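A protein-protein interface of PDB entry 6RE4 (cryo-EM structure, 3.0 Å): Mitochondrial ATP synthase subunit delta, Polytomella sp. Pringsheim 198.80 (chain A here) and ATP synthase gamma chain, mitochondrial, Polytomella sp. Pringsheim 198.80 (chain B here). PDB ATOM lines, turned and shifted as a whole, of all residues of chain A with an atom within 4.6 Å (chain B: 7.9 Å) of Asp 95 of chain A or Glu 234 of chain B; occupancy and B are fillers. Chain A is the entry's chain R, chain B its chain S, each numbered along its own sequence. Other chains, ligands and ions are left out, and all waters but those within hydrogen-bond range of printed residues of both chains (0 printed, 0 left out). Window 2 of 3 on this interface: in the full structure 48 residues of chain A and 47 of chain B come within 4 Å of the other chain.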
ATOM      1  N   GLY A  93       8.115 -11.204 -27.221  1.00  0.00           N
ATOM      2  CA  GLY A  93       7.261 -11.785 -28.240  1.00  0.00           C
ATOM      3  C   GLY A  93       7.899 -11.780 -29.615  1.00  0.00           C
ATOM      4  O   GLY A  93       8.929 -11.157 -29.854  1.00  0.00           O
ATOM      5  N   VAL A  94       7.277 -12.511 -30.545  1.00  0.00           N
ATOM      6  CA  VAL A  94       7.821 -12.581 -31.897  1.00  0.00           C
ATOM      7  C   VAL A  94       7.611 -11.284 -32.652  1.00  0.00           C
ATOM      8  O   VAL A  94       8.280 -11.044 -33.661  1.00  0.00           O
ATOM      9  CB  VAL A  94       7.223 -13.749 -32.692  1.00  0.00           C
ATOM     10  CG1 VAL A  94       7.684 -15.043 -32.120  1.00  0.00           C
ATOM     11  CG2 VAL A  94       5.732 -13.684 -32.656  1.00  0.00           C
ATOM     12  N   ASP A  95       6.689 -10.446 -32.201  1.00  0.00           N
ATOM     13  CA  ASP A  95       6.565  -9.093 -32.703  1.00  0.00           C
ATOM     14  C   ASP A  95       7.141  -8.071 -31.741  1.00  0.00           C
ATOM     15  O   ASP A  95       6.635  -6.955 -31.680  1.00  0.00           O
ATOM     16  CB  ASP A  95       5.105  -8.771 -32.997  1.00  0.00           C
ATOM     17  CG  ASP A  95       4.504  -9.713 -34.003  1.00  0.00           C
ATOM     18  OD1 ASP A  95       5.278 -10.422 -34.667  1.00  0.00           O
ATOM     19  OD2 ASP A  95       3.263  -9.756 -34.128  1.00  0.00           O
ATOM     20  N   GLY A  96       8.136  -8.439 -30.945  1.00  0.00           N
ATOM     21  CA  GLY A  96       8.880  -7.489 -30.145  1.00  0.00           C
ATOM     22  C   GLY A  96       8.639  -7.673 -28.662  1.00  0.00           C
ATOM     23  O   GLY A  96       7.685  -8.312 -28.227  1.00  0.00           O
ATOM     24  N   PHE A  98       7.271  -6.962 -25.393  1.00  0.00           N
ATOM     25  CA  PHE A  98       6.135  -6.247 -24.842  1.00  0.00           C
ATOM     26  C   PHE A  98       6.148  -6.344 -23.327  1.00  0.00           C
ATOM     27  O   PHE A  98       6.876  -7.137 -22.736  1.00  0.00           O
ATOM     28  CB  PHE A  98       4.823  -6.766 -25.434  1.00  0.00           C
ATOM     29  CG  PHE A  98       4.476  -8.167 -25.048  1.00  0.00           C
ATOM     30  CD1 PHE A  98       5.051  -9.243 -25.691  1.00  0.00           C
ATOM     31  CD2 PHE A  98       3.526  -8.406 -24.079  1.00  0.00           C
ATOM     32  CE1 PHE A  98       4.715 -10.524 -25.338  1.00  0.00           C
ATOM     33  CE2 PHE A  98       3.188  -9.684 -23.727  1.00  0.00           C
ATOM     34  CZ  PHE A  98       3.786 -10.737 -24.350  1.00  0.00           C
ATOM     35  N   THR A 107      -3.849 -12.205 -23.607  1.00  0.00           N
ATOM     36  CA  THR A 107      -3.007 -12.371 -24.783  1.00  0.00           C
ATOM     37  C   THR A 107      -2.258 -13.697 -24.741  1.00  0.00           C
ATOM     38  O   THR A 107      -1.546 -13.992 -23.780  1.00  0.00           O
ATOM     39  CB  THR A 107      -2.047 -11.176 -24.933  1.00  0.00           C
ATOM     40  OG1 THR A 107      -1.109 -11.425 -25.980  1.00  0.00           O
ATOM     41  CG2 THR A 107      -1.327 -10.819 -23.647  1.00  0.00           C
ATOM     42  N   ILE A 108      -2.462 -14.523 -25.762  1.00  0.00           N
ATOM     43  CA  ILE A 108      -1.625 -15.692 -26.001  1.00  0.00           C
ATOM     44  C   ILE A 108      -0.494 -15.218 -26.900  1.00  0.00           C
ATOM     45  O   ILE A 108      -0.703 -14.939 -28.076  1.00  0.00           O
ATOM     46  CB  ILE A 108      -2.398 -16.831 -26.654  1.00  0.00           C
ATOM     47  CG1 ILE A 108      -3.536 -17.298 -25.767  1.00  0.00           C
ATOM     48  CG2 ILE A 108      -1.472 -17.962 -26.917  1.00  0.00           C
ATOM     49  CD1 ILE A 108      -4.476 -18.232 -26.476  1.00  0.00           C
ATOM     50  N   ALA A 109       0.704 -15.121 -26.352  1.00  0.00           N
ATOM     51  CA  ALA A 109       1.811 -14.501 -27.061  1.00  0.00           C
ATOM     52  C   ALA A 109       2.903 -15.518 -27.309  1.00  0.00           C
ATOM     53  O   ALA A 109       3.470 -16.058 -26.360  1.00  0.00           O
ATOM     54  CB  ALA A 109       2.367 -13.330 -26.269  1.00  0.00           C
ATOM     55  N   GLN A 110       3.204 -15.772 -28.572  1.00  0.00           N
ATOM     56  CA  GLN A 110       4.349 -16.604 -28.886  1.00  0.00           C
ATOM     57  C   GLN A 110       5.617 -15.804 -28.669  1.00  0.00           C
ATOM     58  O   GLN A 110       5.725 -14.668 -29.132  1.00  0.00           O
ATOM     59  CB  GLN A 110       4.276 -17.101 -30.321  1.00  0.00           C
ATOM     60  CG  GLN A 110       5.365 -18.069 -30.658  1.00  0.00           C
ATOM     61  CD  GLN A 110       5.174 -18.694 -32.006  1.00  0.00           C
ATOM     62  OE1 GLN A 110       4.176 -18.450 -32.676  1.00  0.00           O
ATOM     63  NE2 GLN A 110       6.136 -19.504 -32.420  1.00  0.00           N
ATOM     64  N   TYR B 231      -8.690 -13.721 -25.887  1.00  0.00           N
ATOM     65  CA  TYR B 231      -7.242 -13.672 -25.937  1.00  0.00           C
ATOM     66  C   TYR B 231      -6.790 -13.025 -27.230  1.00  0.00           C
ATOM     67  O   TYR B 231      -7.324 -13.318 -28.301  1.00  0.00           O
ATOM     68  CB  TYR B 231      -6.644 -15.072 -25.837  1.00  0.00           C
ATOM     69  CG  TYR B 231      -6.940 -15.804 -24.556  1.00  0.00           C
ATOM     70  CD1 TYR B 231      -6.008 -15.861 -23.538  1.00  0.00           C
ATOM     71  CD2 TYR B 231      -8.139 -16.461 -24.379  1.00  0.00           C
ATOM     72  CE1 TYR B 231      -6.276 -16.536 -22.381  1.00  0.00           C
ATOM     73  CE2 TYR B 231      -8.414 -17.127 -23.233  1.00  0.00           C
ATOM     74  CZ  TYR B 231      -7.486 -17.166 -22.240  1.00  0.00           C
ATOM     75  OH  TYR B 231      -7.792 -17.856 -21.097  1.00  0.00           O
ATOM     76  N   ASP B 232      -5.797 -12.155 -27.131  1.00  0.00           N
ATOM     77  CA  ASP B 232      -5.241 -11.478 -28.291  1.00  0.00           C
ATOM     78  C   ASP B 232      -4.000 -12.218 -28.751  1.00  0.00           C
ATOM     79  O   ASP B 232      -2.986 -12.223 -28.053  1.00  0.00           O
ATOM     80  CB  ASP B 232      -4.897 -10.030 -27.979  1.00  0.00           C
ATOM     81  CG  ASP B 232      -6.109  -9.207 -27.721  1.00  0.00           C
ATOM     82  OD1 ASP B 232      -7.198  -9.585 -28.195  1.00  0.00           O
ATOM     83  OD2 ASP B 232      -5.973  -8.164 -27.068  1.00  0.00           O
ATOM     84  N   ILE B 233      -4.075 -12.805 -29.931  1.00  0.00           N
ATOM     85  CA  ILE B 233      -3.004 -13.644 -30.440  1.00  0.00           C
ATOM     86  C   ILE B 233      -1.850 -12.760 -30.876  1.00  0.00           C
ATOM     87  O   ILE B 233      -2.029 -11.833 -31.669  1.00  0.00           O
ATOM     88  CB  ILE B 233      -3.501 -14.511 -31.599  1.00  0.00           C
ATOM     89  CG1 ILE B 233      -4.717 -15.315 -31.160  1.00  0.00           C
ATOM     90  CG2 ILE B 233      -2.412 -15.399 -32.079  1.00  0.00           C
ATOM     91  CD1 ILE B 233      -4.480 -16.189 -29.976  1.00  0.00           C
ATOM     92  N   GLU B 234      -0.669 -13.037 -30.355  1.00  0.00           N
ATOM     93  CA  GLU B 234       0.528 -12.280 -30.671  1.00  0.00           C
ATOM     94  C   GLU B 234       1.490 -13.186 -31.432  1.00  0.00           C
ATOM     95  O   GLU B 234       2.707 -13.114 -31.287  1.00  0.00           O
ATOM     96  CB  GLU B 234       1.130 -11.723 -29.387  1.00  0.00           C
ATOM     97  CG  GLU B 234       1.933 -10.433 -29.477  1.00  0.00           C
ATOM     98  CD  GLU B 234       3.422 -10.622 -29.628  1.00  0.00           C
ATOM     99  OE1 GLU B 234       3.961 -11.666 -29.230  1.00  0.00           O
ATOM    100  OE2 GLU B 234       4.074  -9.682 -30.100  1.00  0.00           O
ATOM    101  N   ALA B 235       0.939 -14.076 -32.244  1.00  0.00           N
ATOM    102  CA  ALA B 235       1.746 -14.993 -33.026  1.00  0.00           C
ATOM    103  C   ALA B 235       2.253 -14.321 -34.290  1.00  0.00           C
ATOM    104  O   ALA B 235       1.853 -13.216 -34.647  1.00  0.00           O
ATOM    105  CB  ALA B 235       0.943 -16.236 -33.389  1.00  0.00           C
ATOM    106  N   SER B 236       3.156 -15.014 -34.974  1.00  0.00           N
ATOM    107  CA  SER B 236       3.592 -14.561 -36.286  1.00  0.00           C
ATOM    108  C   SER B 236       2.568 -14.887 -37.358  1.00  0.00           C
ATOM    109  O   SER B 236       2.551 -14.241 -38.406  1.00  0.00           O
ATOM    110  CB  SER B 236       4.927 -15.196 -36.654  1.00  0.00           C
ATOM    111  OG  SER B 236       4.724 -16.471 -37.228  1.00  0.00           O
ATOM    112  N   HIS B 237       1.732 -15.887 -37.131  1.00  0.00           N
ATOM    113  CA  HIS B 237       0.718 -16.302 -38.084  1.00  0.00           C
ATOM    114  C   HIS B 237      -0.629 -16.388 -37.374  1.00  0.00           C
ATOM    115  O   HIS B 237      -0.771 -15.948 -36.234  1.00  0.00           O
ATOM    116  CB  HIS B 237       1.130 -17.610 -38.746  1.00  0.00           C
ATOM    117  CG  HIS B 237       2.276 -17.457 -39.691  1.00  0.00           C
ATOM    118  ND1 HIS B 237       3.563 -17.212 -39.269  1.00  0.00           N
ATOM    119  CD2 HIS B 237       2.328 -17.501 -41.042  1.00  0.00           C
ATOM    120  CE1 HIS B 237       4.361 -17.123 -40.317  1.00  0.00           C
ATOM    121  NE2 HIS B 237       3.636 -17.297 -41.405  1.00  0.00           N
ATOM    122  N   VAL B 242      -1.041 -20.960 -34.227  1.00  0.00           N
ATOM    123  CA  VAL B 242      -0.613 -20.867 -32.838  1.00  0.00           C
ATOM    124  C   VAL B 242      -1.343 -21.893 -31.983  1.00  0.00           C
ATOM    125  O   VAL B 242      -0.780 -22.399 -31.014  1.00  0.00           O
ATOM    126  CB  VAL B 242      -0.770 -19.426 -32.305  1.00  0.00           C
ATOM    127  CG1 VAL B 242      -2.187 -19.086 -31.981  1.00  0.00           C
ATOM    128  CG2 VAL B 242       0.077 -19.218 -31.082  1.00  0.00           C
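Of chain B, only Glu 234 and Ala 235 come within 4 Å of Asp 95 of chain A. Of chain A, only Gly 93 (3.4 Å), Val 94 (3.4 Å), Asp 95 (3.2 Å), Ile 108 (3.0 Å), Ala 109 (3.7 Å) and Gln 110 (3.5 Å) come within 4 Å of Glu 234 of chain B. No residue of chain B comes within 4 Å of Gly 96 of chain A. Of the printed residues of chain B, Val 94 of chain A touches Glu 234, Ala 235 and Ser 236. Printed residues of chain A within 4 Å of Asp 232 of chain B: Thr 107 and Ile 108. Of the printed residues of chain A, Ser 236 of chain B touches Val 94. Of the printed residues of chain B, Ala 109 of chain A touches Glu 234 (3.7 Å). Of the printed residues of chain B, Thr 107 of chain A touches Asp 232 (2.9 Å).
Hydrophobic or aromatic side chains of chain A that line the printed part of chain B: Val 94, Ile 108 and Ala 109. Among the printed residues, no Asp or Glu carboxylate lies within 4 Å of a Lys or Arg side-chain nitrogen of the other chain.
CA of Gly 93 of chain A touches OE1 of Glu 234 of chain B, at 3.4 Å. CG2 of Val 94 of chain A touches O of Glu 234 of chain B, at 3.4 Å. C of Ala 235 of chain B touches CG2 of Val 94 of chain A, 3.9 Å away. CG2 of Val 94 of chain A touches N of Ser 236 of chain B (3.7 Å). Ala 235 of chain B touches Asp 95 of chain A (O to OD2, 3.8 Å). Ile 108 of chain A touches Tyr 231 of chain B. O of Ile 108 of chain A touches CA of Ile 233 of chain B, 3.5 Å away. Ala 109 of chain A touches Glu 234 of chain B (CA to CB, 3.7 Å). Ala 235 of chain B touches Gln 110 of chain A (CB to OE1, 3.98 Å).
The backbone NH (N) of Val 94 of chain A lies within hydrogen-bond range of the backbone carbonyl oxygen (O) of Gln 110 of chain A, at 3.0 Å. ND1 of His 237 of chain B lies within hydrogen-bond range of OG of Ser 236 of chain B, at 2.5 Å.
The side-chain carboxylate of Glu 234 of chain B sits close to the backbone NH of Asp 95 of chain A, 3.4 Å away. The side-chain carboxylate (OE1) of Glu 234 of chain B sits close to the backbone carbonyl oxygen (O) of Gln 110 of chain A (3.5 Å). O of Ile 108 of chain A sits at hydrogen-bond distance from N of Glu 234 of chain B, 3.0 Å away. O of Asp 232 of chain B is in hydrogen-bond range of OG1 of Thr 107 of chain A (2.9 Å). The backbone NH (N) of Ile 108 of chain A sits at hydrogen-bond distance from the backbone carbonyl oxygen (O) of Asp 232 of chain B, at 3.3 Å.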
